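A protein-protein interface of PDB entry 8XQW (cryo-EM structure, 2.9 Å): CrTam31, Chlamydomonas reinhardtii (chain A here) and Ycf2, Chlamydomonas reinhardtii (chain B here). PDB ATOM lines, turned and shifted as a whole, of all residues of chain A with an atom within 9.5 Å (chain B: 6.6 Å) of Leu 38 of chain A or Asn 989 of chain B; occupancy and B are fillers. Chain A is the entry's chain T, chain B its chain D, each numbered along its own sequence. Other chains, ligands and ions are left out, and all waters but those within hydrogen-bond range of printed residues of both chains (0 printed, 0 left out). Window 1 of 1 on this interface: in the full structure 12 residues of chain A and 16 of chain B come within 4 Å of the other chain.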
ATOM      1  N   SEP A  18      27.583  32.374  12.907  1.00  0.00           N
ATOM      2  CA  SEP A  18      27.696  33.257  14.064  1.00  0.00           C
ATOM      3  CB  SEP A  18      26.544  32.995  15.033  1.00  0.00           C
ATOM      4  OG  SEP A  18      26.567  31.651  15.473  1.00  0.00           O
ATOM      5  C   SEP A  18      29.019  33.128  14.816  1.00  0.00           C
ATOM      6  O   SEP A  18      29.635  34.132  15.168  1.00  0.00           O
ATOM      7  P   SEP A  18      25.442  31.378  16.588  1.00  0.00           P
ATOM      8  O1P SEP A  18      25.569  29.857  17.095  1.00  0.00           O
ATOM      9  O2P SEP A  18      23.985  31.617  15.947  1.00  0.00           O
ATOM     10  O3P SEP A  18      25.665  32.363  17.842  1.00  0.00           O
ATOM     11  N   VAL A  19      29.446  31.896  15.072  1.00  0.00           N
ATOM     12  CA  VAL A  19      30.633  31.658  15.885  1.00  0.00           C
ATOM     13  C   VAL A  19      31.874  32.199  15.177  1.00  0.00           C
ATOM     14  O   VAL A  19      32.813  32.670  15.821  1.00  0.00           O
ATOM     15  CB  VAL A  19      30.781  30.158  16.215  1.00  0.00           C
ATOM     16  CG1 VAL A  19      30.696  29.324  14.954  1.00  0.00           C
ATOM     17  CG2 VAL A  19      32.078  29.889  16.958  1.00  0.00           C
ATOM     18  N   SER A  31      40.184  25.016  16.436  1.00  0.00           N
ATOM     19  CA  SER A  31      39.382  25.462  17.566  1.00  0.00           C
ATOM     20  C   SER A  31      37.991  25.900  17.130  1.00  0.00           C
ATOM     21  O   SER A  31      37.041  25.832  17.922  1.00  0.00           O
ATOM     22  CB  SER A  31      40.101  26.585  18.300  1.00  0.00           C
ATOM     23  OG  SER A  31      41.327  26.118  18.831  1.00  0.00           O
ATOM     24  N   LEU A  32      37.831  26.309  15.873  1.00  0.00           N
ATOM     25  CA  LEU A  32      36.506  26.705  15.415  1.00  0.00           C
ATOM     26  C   LEU A  32      35.593  25.491  15.281  1.00  0.00           C
ATOM     27  O   LEU A  32      34.446  25.519  15.738  1.00  0.00           O
ATOM     28  CB  LEU A  32      36.612  27.468  14.098  1.00  0.00           C
ATOM     29  CG  LEU A  32      35.728  28.715  14.029  1.00  0.00           C
ATOM     30  CD1 LEU A  32      36.174  29.641  12.911  1.00  0.00           C
ATOM     31  CD2 LEU A  32      34.271  28.349  13.866  1.00  0.00           C
ATOM     32  N   GLU A  33      36.087  24.406  14.681  1.00  0.00           N
ATOM     33  CA  GLU A  33      35.311  23.169  14.664  1.00  0.00           C
ATOM     34  C   GLU A  33      35.153  22.599  16.064  1.00  0.00           C
ATOM     35  O   GLU A  33      34.134  21.972  16.370  1.00  0.00           O
ATOM     36  CB  GLU A  33      35.970  22.143  13.746  1.00  0.00           C
ATOM     37  CG  GLU A  33      36.064  22.599  12.309  1.00  0.00           C
ATOM     38  CD  GLU A  33      34.903  23.486  11.920  1.00  0.00           C
ATOM     39  OE1 GLU A  33      33.803  22.950  11.671  1.00  0.00           O
ATOM     40  OE2 GLU A  33      35.088  24.720  11.869  1.00  0.00           O
ATOM     41  N   TYR A  34      36.154  22.803  16.918  1.00  0.00           N
ATOM     42  CA  TYR A  34      36.035  22.453  18.327  1.00  0.00           C
ATOM     43  C   TYR A  34      34.798  23.093  18.941  1.00  0.00           C
ATOM     44  O   TYR A  34      34.012  22.428  19.622  1.00  0.00           O
ATOM     45  CB  TYR A  34      37.303  22.904  19.043  1.00  0.00           C
ATOM     46  CG  TYR A  34      37.465  22.490  20.479  1.00  0.00           C
ATOM     47  CD1 TYR A  34      36.719  23.081  21.483  1.00  0.00           C
ATOM     48  CD2 TYR A  34      38.415  21.551  20.835  1.00  0.00           C
ATOM     49  CE1 TYR A  34      36.890  22.722  22.794  1.00  0.00           C
ATOM     50  CE2 TYR A  34      38.595  21.186  22.143  1.00  0.00           C
ATOM     51  CZ  TYR A  34      37.831  21.775  23.118  1.00  0.00           C
ATOM     52  OH  TYR A  34      38.020  21.407  24.426  1.00  0.00           O
ATOM     53  N   ILE A  35      34.605  24.387  18.698  1.00  0.00           N
ATOM     54  CA  ILE A  35      33.459  25.088  19.270  1.00  0.00           C
ATOM     55  C   ILE A  35      32.168  24.755  18.521  1.00  0.00           C
ATOM     56  O   ILE A  35      31.076  24.815  19.098  1.00  0.00           O
ATOM     57  CB  ILE A  35      33.734  26.605  19.292  1.00  0.00           C
ATOM     58  CG1 ILE A  35      34.888  26.928  20.241  1.00  0.00           C
ATOM     59  CG2 ILE A  35      32.512  27.390  19.726  1.00  0.00           C
ATOM     60  CD1 ILE A  35      34.846  26.159  21.541  1.00  0.00           C
ATOM     61  N   ARG A  36      32.262  24.390  17.244  1.00  0.00           N
ATOM     62  CA  ARG A  36      31.059  24.190  16.443  1.00  0.00           C
ATOM     63  C   ARG A  36      30.308  22.910  16.787  1.00  0.00           C
ATOM     64  O   ARG A  36      29.134  22.790  16.429  1.00  0.00           O
ATOM     65  CB  ARG A  36      31.406  24.172  14.956  1.00  0.00           C
ATOM     66  CG  ARG A  36      31.331  25.518  14.265  1.00  0.00           C
ATOM     67  CD  ARG A  36      32.144  25.485  12.982  1.00  0.00           C
ATOM     68  NE  ARG A  36      31.941  26.669  12.155  1.00  0.00           N
ATOM     69  CZ  ARG A  36      32.708  26.990  11.118  1.00  0.00           C
ATOM     70  NH1 ARG A  36      33.733  26.223  10.785  1.00  0.00           N
ATOM     71  NH2 ARG A  36      32.455  28.083  10.418  1.00  0.00           N
ATOM     72  N   ALA A  37      30.946  21.950  17.445  1.00  0.00           N
ATOM     73  CA  ALA A  37      30.316  20.656  17.679  1.00  0.00           C
ATOM     74  C   ALA A  37      29.883  20.444  19.123  1.00  0.00           C
ATOM     75  O   ALA A  37      30.038  19.331  19.631  1.00  0.00           O
ATOM     76  CB  ALA A  37      31.259  19.528  17.254  1.00  0.00           C
ATOM     77  N   LEU A  38      29.346  21.462  19.796  1.00  0.00           N
ATOM     78  CA  LEU A  38      29.002  21.344  21.208  1.00  0.00           C
ATOM     79  C   LEU A  38      27.642  21.932  21.562  1.00  0.00           C
ATOM     80  O   LEU A  38      27.271  21.920  22.740  1.00  0.00           O
ATOM     81  CB  LEU A  38      30.082  22.002  22.066  1.00  0.00           C
ATOM     82  CG  LEU A  38      31.332  21.161  22.304  1.00  0.00           C
ATOM     83  CD1 LEU A  38      32.353  21.937  23.094  1.00  0.00           C
ATOM     84  CD2 LEU A  38      30.969  19.889  23.024  1.00  0.00           C
ATOM     85  N   GLY A  39      26.887  22.441  20.593  1.00  0.00           N
ATOM     86  CA  GLY A  39      25.602  23.038  20.880  1.00  0.00           C
ATOM     87  C   GLY A  39      25.397  24.332  20.123  1.00  0.00           C
ATOM     88  O   GLY A  39      26.358  24.996  19.731  1.00  0.00           O
ATOM     89  N   PRO A  40      24.132  24.709  19.882  1.00  0.00           N
ATOM     90  CA  PRO A  40      23.869  25.811  18.946  1.00  0.00           C
ATOM     91  C   PRO A  40      24.444  27.154  19.376  1.00  0.00           C
ATOM     92  O   PRO A  40      25.416  27.618  18.769  1.00  0.00           O
ATOM     93  CB  PRO A  40      22.335  25.863  18.895  1.00  0.00           C
ATOM     94  CG  PRO A  40      21.880  24.556  19.447  1.00  0.00           C
ATOM     95  CD  PRO A  40      22.895  24.171  20.459  1.00  0.00           C
ATOM     96  N   LYS A  41      23.878  27.806  20.394  1.00  0.00           N
ATOM     97  CA  LYS A  41      24.658  28.809  21.107  1.00  0.00           C
ATOM     98  C   LYS A  41      24.548  28.693  22.620  1.00  0.00           C
ATOM     99  O   LYS A  41      25.498  28.319  23.310  1.00  0.00           O
ATOM    100  CB  LYS A  41      24.216  30.202  20.659  1.00  0.00           C
ATOM    101  CG  LYS A  41      24.815  31.352  21.454  1.00  0.00           C
ATOM    102  CD  LYS A  41      24.351  32.678  20.888  1.00  0.00           C
ATOM    103  CE  LYS A  41      22.853  32.667  20.634  1.00  0.00           C
ATOM    104  NZ  LYS A  41      22.088  32.443  21.890  1.00  0.00           N
ATOM    105  N   LYS A  42      23.360  29.012  23.126  1.00  0.00           N
ATOM    106  CA  LYS A  42      23.035  28.942  24.540  1.00  0.00           C
ATOM    107  C   LYS A  42      21.522  29.026  24.668  1.00  0.00           C
ATOM    108  O   LYS A  42      20.958  30.121  24.596  1.00  0.00           O
ATOM    109  CB  LYS A  42      23.732  30.066  25.304  1.00  0.00           C
ATOM    110  CG  LYS A  42      23.656  29.962  26.805  1.00  0.00           C
ATOM    111  CD  LYS A  42      24.624  30.939  27.441  1.00  0.00           C
ATOM    112  CE  LYS A  42      24.605  30.851  28.950  1.00  0.00           C
ATOM    113  NZ  LYS A  42      25.827  31.448  29.549  1.00  0.00           N
ATOM    114  N   GLY A  43      20.848  27.899  24.860  1.00  0.00           N
ATOM    115  CA  GLY A  43      19.404  27.917  24.764  1.00  0.00           C
ATOM    116  C   GLY A  43      18.665  27.487  26.011  1.00  0.00           C
ATOM    117  O   GLY A  43      19.003  27.900  27.124  1.00  0.00           O
ATOM    118  N   ALA A  44      17.645  26.654  25.819  1.00  0.00           N
ATOM    119  CA  ALA A  44      16.808  26.231  26.936  1.00  0.00           C
ATOM    120  C   ALA A  44      17.574  25.562  28.070  1.00  0.00           C
ATOM    121  O   ALA A  44      17.297  25.897  29.234  1.00  0.00           O
ATOM    122  CB  ALA A  44      15.695  25.313  26.418  1.00  0.00           C
ATOM    123  N   PRO A  45      18.516  24.642  27.834  1.00  0.00           N
ATOM    124  CA  PRO A  45      19.231  24.029  28.964  1.00  0.00           C
ATOM    125  C   PRO A  45      19.990  25.020  29.821  1.00  0.00           C
ATOM    126  O   PRO A  45      20.317  24.690  30.967  1.00  0.00           O
ATOM    127  CB  PRO A  45      20.194  23.050  28.286  1.00  0.00           C
ATOM    128  CG  PRO A  45      19.604  22.789  26.972  1.00  0.00           C
ATOM    129  CD  PRO A  45      18.940  24.049  26.556  1.00  0.00           C
ATOM    130  N   PHE A  46      20.272  26.219  29.316  1.00  0.00           N
ATOM    131  CA  PHE A  46      21.078  27.201  30.026  1.00  0.00           C
ATOM    132  C   PHE A  46      20.268  28.440  30.383  1.00  0.00           C
ATOM    133  O   PHE A  46      20.809  29.544  30.439  1.00  0.00           O
ATOM    134  CB  PHE A  46      22.308  27.578  29.206  1.00  0.00           C
ATOM    135  CG  PHE A  46      23.308  26.474  29.085  1.00  0.00           C
ATOM    136  CD1 PHE A  46      23.140  25.474  28.150  1.00  0.00           C
ATOM    137  CD2 PHE A  46      24.412  26.427  29.909  1.00  0.00           C
ATOM    138  CE1 PHE A  46      24.054  24.456  28.039  1.00  0.00           C
ATOM    139  CE2 PHE A  46      25.328  25.410  29.801  1.00  0.00           C
ATOM    140  CZ  PHE A  46      25.148  24.424  28.867  1.00  0.00           C
ATOM    141  N   ASP A  50      15.277  29.950  23.358  1.00  0.00           N
ATOM    142  CA  ASP A  50      15.701  29.405  22.081  1.00  0.00           C
ATOM    143  C   ASP A  50      15.390  30.385  20.953  1.00  0.00           C
ATOM    144  O   ASP A  50      14.451  31.181  21.049  1.00  0.00           O
ATOM    145  CB  ASP A  50      15.001  28.077  21.809  1.00  0.00           C
ATOM    146  CG  ASP A  50      15.921  26.891  21.958  1.00  0.00           C
ATOM    147  OD1 ASP A  50      17.154  27.089  22.006  1.00  0.00           O
ATOM    148  OD2 ASP A  50      15.408  25.757  22.022  1.00  0.00           O
ATOM    149  N   THR B 879      26.021  24.270  13.762  1.00  0.00           N
ATOM    150  CA  THR B 879      26.331  23.842  15.124  1.00  0.00           C
ATOM    151  C   THR B 879      25.296  22.807  15.551  1.00  0.00           C
ATOM    152  O   THR B 879      24.166  23.146  15.903  1.00  0.00           O
ATOM    153  CB  THR B 879      26.369  25.035  16.069  1.00  0.00           C
ATOM    154  OG1 THR B 879      25.378  25.994  15.677  1.00  0.00           O
ATOM    155  CG2 THR B 879      27.735  25.694  16.024  1.00  0.00           C
ATOM    156  N   SER B 880      25.686  21.536  15.499  1.00  0.00           N
ATOM    157  CA  SER B 880      24.885  20.424  15.979  1.00  0.00           C
ATOM    158  C   SER B 880      25.774  19.504  16.800  1.00  0.00           C
ATOM    159  O   SER B 880      26.896  19.195  16.390  1.00  0.00           O
ATOM    160  CB  SER B 880      24.254  19.651  14.820  1.00  0.00           C
ATOM    161  OG  SER B 880      23.511  18.545  15.295  1.00  0.00           O
ATOM    162  N   LEU B 881      25.277  19.070  17.957  1.00  0.00           N
ATOM    163  CA  LEU B 881      26.079  18.259  18.866  1.00  0.00           C
ATOM    164  C   LEU B 881      26.489  16.950  18.207  1.00  0.00           C
ATOM    165  O   LEU B 881      25.652  16.074  17.977  1.00  0.00           O
ATOM    166  CB  LEU B 881      25.307  17.987  20.156  1.00  0.00           C
ATOM    167  CG  LEU B 881      25.987  17.126  21.215  1.00  0.00           C
ATOM    168  CD1 LEU B 881      27.417  17.559  21.417  1.00  0.00           C
ATOM    169  CD2 LEU B 881      25.219  17.215  22.516  1.00  0.00           C
ATOM    170  N   ARG B 882      27.774  16.812  17.891  1.00  0.00           N
ATOM    171  CA  ARG B 882      28.276  15.622  17.222  1.00  0.00           C
ATOM    172  C   ARG B 882      29.593  15.097  17.765  1.00  0.00           C
ATOM    173  O   ARG B 882      29.956  13.965  17.430  1.00  0.00           O
ATOM    174  CB  ARG B 882      28.444  15.889  15.721  1.00  0.00           C
ATOM    175  CG  ARG B 882      29.727  16.601  15.369  1.00  0.00           C
ATOM    176  CD  ARG B 882      29.668  17.137  13.953  1.00  0.00           C
ATOM    177  NE  ARG B 882      28.538  18.040  13.773  1.00  0.00           N
ATOM    178  CZ  ARG B 882      28.624  19.362  13.859  1.00  0.00           C
ATOM    179  NH1 ARG B 882      27.546  20.110  13.684  1.00  0.00           N
ATOM    180  NH2 ARG B 882      29.791  19.934  14.119  1.00  0.00           N
ATOM    181  N   GLY B 883      30.317  15.858  18.571  1.00  0.00           N
ATOM    182  CA  GLY B 883      31.617  15.435  19.041  1.00  0.00           C
ATOM    183  C   GLY B 883      32.651  15.395  17.928  1.00  0.00           C
ATOM    184  O   GLY B 883      32.338  15.301  16.744  1.00  0.00           O
ATOM    185  N   PHE B 887      38.485  16.470  21.385  1.00  0.00           N
ATOM    186  CA  PHE B 887      38.331  16.168  22.801  1.00  0.00           C
ATOM    187  C   PHE B 887      38.812  14.744  23.021  1.00  0.00           C
ATOM    188  O   PHE B 887      38.072  13.792  22.762  1.00  0.00           O
ATOM    189  CB  PHE B 887      36.886  16.314  23.267  1.00  0.00           C
ATOM    190  CG  PHE B 887      36.019  17.153  22.373  1.00  0.00           C
ATOM    191  CD1 PHE B 887      36.378  18.431  22.006  1.00  0.00           C
ATOM    192  CD2 PHE B 887      34.804  16.663  21.937  1.00  0.00           C
ATOM    193  CE1 PHE B 887      35.559  19.182  21.190  1.00  0.00           C
ATOM    194  CE2 PHE B 887      33.984  17.414  21.134  1.00  0.00           C
ATOM    195  CZ  PHE B 887      34.359  18.672  20.760  1.00  0.00           C
ATOM    196  N   LEU B 982      33.700  19.855  29.170  1.00  0.00           N
ATOM    197  CA  LEU B 982      33.308  19.274  27.892  1.00  0.00           C
ATOM    198  C   LEU B 982      32.226  18.222  28.074  1.00  0.00           C
ATOM    199  O   LEU B 982      31.194  18.244  27.394  1.00  0.00           O
ATOM    200  CB  LEU B 982      34.527  18.655  27.217  1.00  0.00           C
ATOM    201  CG  LEU B 982      35.006  19.237  25.897  1.00  0.00           C
ATOM    202  CD1 LEU B 982      34.535  20.660  25.732  1.00  0.00           C
ATOM    203  CD2 LEU B 982      36.509  19.158  25.857  1.00  0.00           C
ATOM    204  N   PHE B 984      30.248  17.627  30.703  1.00  0.00           N
ATOM    205  CA  PHE B 984      29.013  18.221  31.205  1.00  0.00           C
ATOM    206  C   PHE B 984      28.228  18.880  30.078  1.00  0.00           C
ATOM    207  O   PHE B 984      27.009  18.698  29.961  1.00  0.00           O
ATOM    208  CB  PHE B 984      29.319  19.231  32.305  1.00  0.00           C
ATOM    209  CG  PHE B 984      28.125  20.011  32.750  1.00  0.00           C
ATOM    210  CD1 PHE B 984      27.273  19.505  33.706  1.00  0.00           C
ATOM    211  CD2 PHE B 984      27.851  21.250  32.209  1.00  0.00           C
ATOM    212  CE1 PHE B 984      26.170  20.218  34.114  1.00  0.00           C
ATOM    213  CE2 PHE B 984      26.751  21.964  32.613  1.00  0.00           C
ATOM    214  CZ  PHE B 984      25.909  21.447  33.565  1.00  0.00           C
ATOM    215  N   LEU B 985      28.919  19.644  29.231  1.00  0.00           N
ATOM    216  CA  LEU B 985      28.246  20.356  28.154  1.00  0.00           C
ATOM    217  C   LEU B 985      27.606  19.395  27.171  1.00  0.00           C
ATOM    218  O   LEU B 985      26.477  19.619  26.723  1.00  0.00           O
ATOM    219  CB  LEU B 985      29.239  21.259  27.430  1.00  0.00           C
ATOM    220  CG  LEU B 985      29.452  22.624  28.058  1.00  0.00           C
ATOM    221  CD1 LEU B 985      30.724  23.235  27.524  1.00  0.00           C
ATOM    222  CD2 LEU B 985      28.271  23.500  27.751  1.00  0.00           C
ATOM    223  N   THR B 986      28.317  18.332  26.803  1.00  0.00           N
ATOM    224  CA  THR B 986      27.751  17.367  25.867  1.00  0.00           C
ATOM    225  C   THR B 986      26.487  16.736  26.429  1.00  0.00           C
ATOM    226  O   THR B 986      25.446  16.694  25.755  1.00  0.00           O
ATOM    227  CB  THR B 986      28.779  16.288  25.541  1.00  0.00           C
ATOM    228  OG1 THR B 986      30.046  16.900  25.289  1.00  0.00           O
ATOM    229  CG2 THR B 986      28.356  15.513  24.318  1.00  0.00           C
ATOM    230  N   GLU B 987      26.554  16.252  27.670  1.00  0.00           N
ATOM    231  CA  GLU B 987      25.394  15.573  28.228  1.00  0.00           C
ATOM    232  C   GLU B 987      24.227  16.514  28.480  1.00  0.00           C
ATOM    233  O   GLU B 987      23.077  16.070  28.440  1.00  0.00           O
ATOM    234  CB  GLU B 987      25.777  14.834  29.509  1.00  0.00           C
ATOM    235  CG  GLU B 987      27.092  14.061  29.426  1.00  0.00           C
ATOM    236  CD  GLU B 987      27.296  13.313  28.114  1.00  0.00           C
ATOM    237  OE1 GLU B 987      28.464  13.143  27.704  1.00  0.00           O
ATOM    238  OE2 GLU B 987      26.305  12.831  27.522  1.00  0.00           O
ATOM    239  N   ARG B 988      24.476  17.797  28.723  1.00  0.00           N
ATOM    240  CA  ARG B 988      23.359  18.722  28.854  1.00  0.00           C
ATOM    241  C   ARG B 988      22.810  19.189  27.517  1.00  0.00           C
ATOM    242  O   ARG B 988      21.614  19.475  27.422  1.00  0.00           O
ATOM    243  CB  ARG B 988      23.767  19.936  29.680  1.00  0.00           C
ATOM    244  CG  ARG B 988      23.517  19.753  31.148  1.00  0.00           C
ATOM    245  CD  ARG B 988      22.546  20.777  31.653  1.00  0.00           C
ATOM    246  NE  ARG B 988      21.334  20.839  30.848  1.00  0.00           N
ATOM    247  CZ  ARG B 988      20.111  20.734  31.349  1.00  0.00           C
ATOM    248  NH1 ARG B 988      19.947  20.562  32.647  1.00  0.00           N
ATOM    249  NH2 ARG B 988      19.051  20.800  30.562  1.00  0.00           N
ATOM    250  N   ASN B 989      23.644  19.275  26.490  1.00  0.00           N
ATOM    251  CA  ASN B 989      23.205  19.723  25.181  1.00  0.00           C
ATOM    252  C   ASN B 989      22.585  18.607  24.365  1.00  0.00           C
ATOM    253  O   ASN B 989      22.079  18.869  23.268  1.00  0.00           O
ATOM    254  CB  ASN B 989      24.378  20.326  24.412  1.00  0.00           C
ATOM    255  CG  ASN B 989      24.717  21.718  24.875  1.00  0.00           C
ATOM    256  OD1 ASN B 989      23.923  22.643  24.726  1.00  0.00           O
ATOM    257  ND2 ASN B 989      25.901  21.877  25.449  1.00  0.00           N
ATOM    258  N   LYS B 990      22.627  17.372  24.860  1.00  0.00           N
ATOM    259  CA  LYS B 990      21.842  16.305  24.246  1.00  0.00           C
ATOM    260  C   LYS B 990      20.354  16.648  24.181  1.00  0.00           C
ATOM    261  O   LYS B 990      19.589  15.961  23.500  1.00  0.00           O
ATOM    262  CB  LYS B 990      22.030  14.992  25.006  1.00  0.00           C
ATOM    263  CG  LYS B 990      22.833  13.957  24.254  1.00  0.00           C
ATOM    264  CD  LYS B 990      23.258  12.828  25.163  1.00  0.00           C
ATOM    265  CE  LYS B 990      24.471  12.115  24.605  1.00  0.00           C
ATOM    266  NZ  LYS B 990      25.227  11.400  25.662  1.00  0.00           N
ATOM    267  N   TYR B 991      19.940  17.709  24.880  1.00  0.00           N
ATOM    268  CA  TYR B 991      18.537  18.116  24.892  1.00  0.00           C
ATOM    269  C   TYR B 991      18.024  18.440  23.496  1.00  0.00           C
ATOM    270  O   TYR B 991      16.831  18.268  23.225  1.00  0.00           O
ATOM    271  CB  TYR B 991      18.355  19.324  25.813  1.00  0.00           C
ATOM    272  CG  TYR B 991      17.097  20.143  25.583  1.00  0.00           C
ATOM    273  CD1 TYR B 991      17.046  21.124  24.609  1.00  0.00           C
ATOM    274  CD2 TYR B 991      15.975  19.958  26.369  1.00  0.00           C
ATOM    275  CE1 TYR B 991      15.911  21.869  24.401  1.00  0.00           C
ATOM    276  CE2 TYR B 991      14.833  20.707  26.170  1.00  0.00           C
ATOM    277  CZ  TYR B 991      14.809  21.660  25.185  1.00  0.00           C
ATOM    278  OH  TYR B 991      13.681  22.412  24.980  1.00  0.00           O
ATOM    279  N   TYR B 992      18.884  18.927  22.612  1.00  0.00           N
ATOM    280  CA  TYR B 992      18.470  19.373  21.292  1.00  0.00           C
ATOM    281  C   TYR B 992      18.511  18.269  20.250  1.00  0.00           C
ATOM    282  O   TYR B 992      18.363  18.556  19.060  1.00  0.00           O
ATOM    283  CB  TYR B 992      19.349  20.534  20.831  1.00  0.00           C
ATOM    284  CG  TYR B 992      19.029  21.829  21.521  1.00  0.00           C
ATOM    285  CD1 TYR B 992      17.913  22.562  21.167  1.00  0.00           C
ATOM    286  CD2 TYR B 992      19.842  22.317  22.530  1.00  0.00           C
ATOM    287  CE1 TYR B 992      17.615  23.740  21.792  1.00  0.00           C
ATOM    288  CE2 TYR B 992      19.550  23.495  23.162  1.00  0.00           C
ATOM    289  CZ  TYR B 992      18.433  24.203  22.790  1.00  0.00           C
ATOM    290  OH  TYR B 992      18.129  25.386  23.417  1.00  0.00           O
ATOM    291  N   LEU B 993      18.703  17.020  20.663  1.00  0.00           N
ATOM    292  CA  LEU B 993      18.888  15.946  19.700  1.00  0.00           C
ATOM    293  C   LEU B 993      17.581  15.357  19.193  1.00  0.00           C
ATOM    294  O   LEU B 993      17.616  14.442  18.366  1.00  0.00           O
ATOM    295  CB  LEU B 993      19.743  14.842  20.313  1.00  0.00           C
ATOM    296  CG  LEU B 993      21.236  15.136  20.293  1.00  0.00           C
ATOM    297  CD1 LEU B 993      22.027  13.889  20.625  1.00  0.00           C
ATOM    298  CD2 LEU B 993      21.639  15.680  18.941  1.00  0.00           C
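The side-chain hydroxyl of Tyr 992 of chain B lies within hydrogen-bond range of the backbone NH of Ala 44 of chain A (2.8 Å).
The side-chain hydroxyl of Tyr 992 of chain B is in hydrogen-bond range of the side-chain carboxylate of Asp 50 of chain A (2.4 Å).
The backbone carbonyl oxygen (O) of Pro 40 of chain A lies within hydrogen-bond range of the side-chain hydroxyl (OG1) of Thr 879 of chain B.
The backbone carbonyl oxygen (O) of Leu 38 of chain A lies within hydrogen-bond range of the side-chain amide nitrogen (ND2) of Asn 989 of chain B (3.0 Å).
The backbone carbonyl oxygen (O) of Leu 982 of chain B lies within hydrogen-bond range of the side-chain hydroxyl (OG1) of Thr 986 of chain B (2.7 Å).
O of Leu 985 of chain B sits at hydrogen-bond distance from ND2 of Asn 989 of chain B, at 2.7 Å.
O of Ser 880 of chain B lies within hydrogen-bond range of NH1 of Arg 882 of chain B, 2.9 Å away.
O1P of SEP 18 of chain A lies close to O of Pro 40 of chain A (2.8 Å).
The side-chain carboxylate (OE1) of Glu 33 of chain A lies within salt-bridge range of the guanidinium group (NH1) of Arg 36 of chain A (3.4 Å).
Tyr 34 of chain A touches Leu 982 of chain B (OH to CD2, 3.1 Å).
Arg 36 of chain A touches Ser 880 of chain B.
Ala 37 of chain A touches Ser 880 of chain B (CA to O, 3.9 Å).
Ala 37 of chain A touches Arg 882 of chain B.
Leu 982 of chain B touches Leu 38 of chain A.
Thr 879 of chain B touches Gly 39 of chain A (CB to O, 3.7 Å).
Gly 43 of chain A touches Tyr 992 of chain B (CA to OH, 3.1 Å).
Pro 45 of chain A touches Tyr 991 of chain B (CG to CD1, 3.9 Å).
CD of Pro 45 of chain A touches CE2 of Tyr 992 of chain B, 3.5 Å away.
CE1 of Phe 46 of chain A touches OD1 of Asn 989 of chain B, at 3.8 Å.
Leu 38 of chain A touches just these residues of chain B: Leu 982 (3.7 Å), Thr 986 (3.9 Å) and Asn 989 (3.0 Å).
Printed residues of chain A within 4 Å of Asn 989 of chain B: Leu 38 and Phe 46.
Printed residues of chain A within 4 Å of Thr 986 of chain B: Leu 38.
Of the printed residues of chain B, Gly 43 of chain A touches Tyr 992.
Of the printed residues of chain B, Pro 40 of chain A touches Thr 879 (3.5 Å).
Of the printed residues of chain B, Phe 46 of chain A touches Leu 985 and Asn 989.
Printed residues of chain A within 4 Å of Ser 880 of chain B: Arg 36 and Ala 37.
Phe 984 of chain B touches none of the printed residues of chain A.
The nearest residue of chain A that does not touch Asn 989 of chain B is Gly 39 of chain A (4.2 Å).
The nearest printed residue of chain B that does not touch Pro 45 of chain A is Asn 989 of chain B (4.9 Å).
Of the 19 printed residues of chain A, 11 touch a printed residue of chain B.
Hydrophobic or aromatic side chains of chain A within 4 Å of the printed part of chain B: Tyr 34, Ala 37, Leu 38, Ala 44, Pro 45 and Phe 46.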
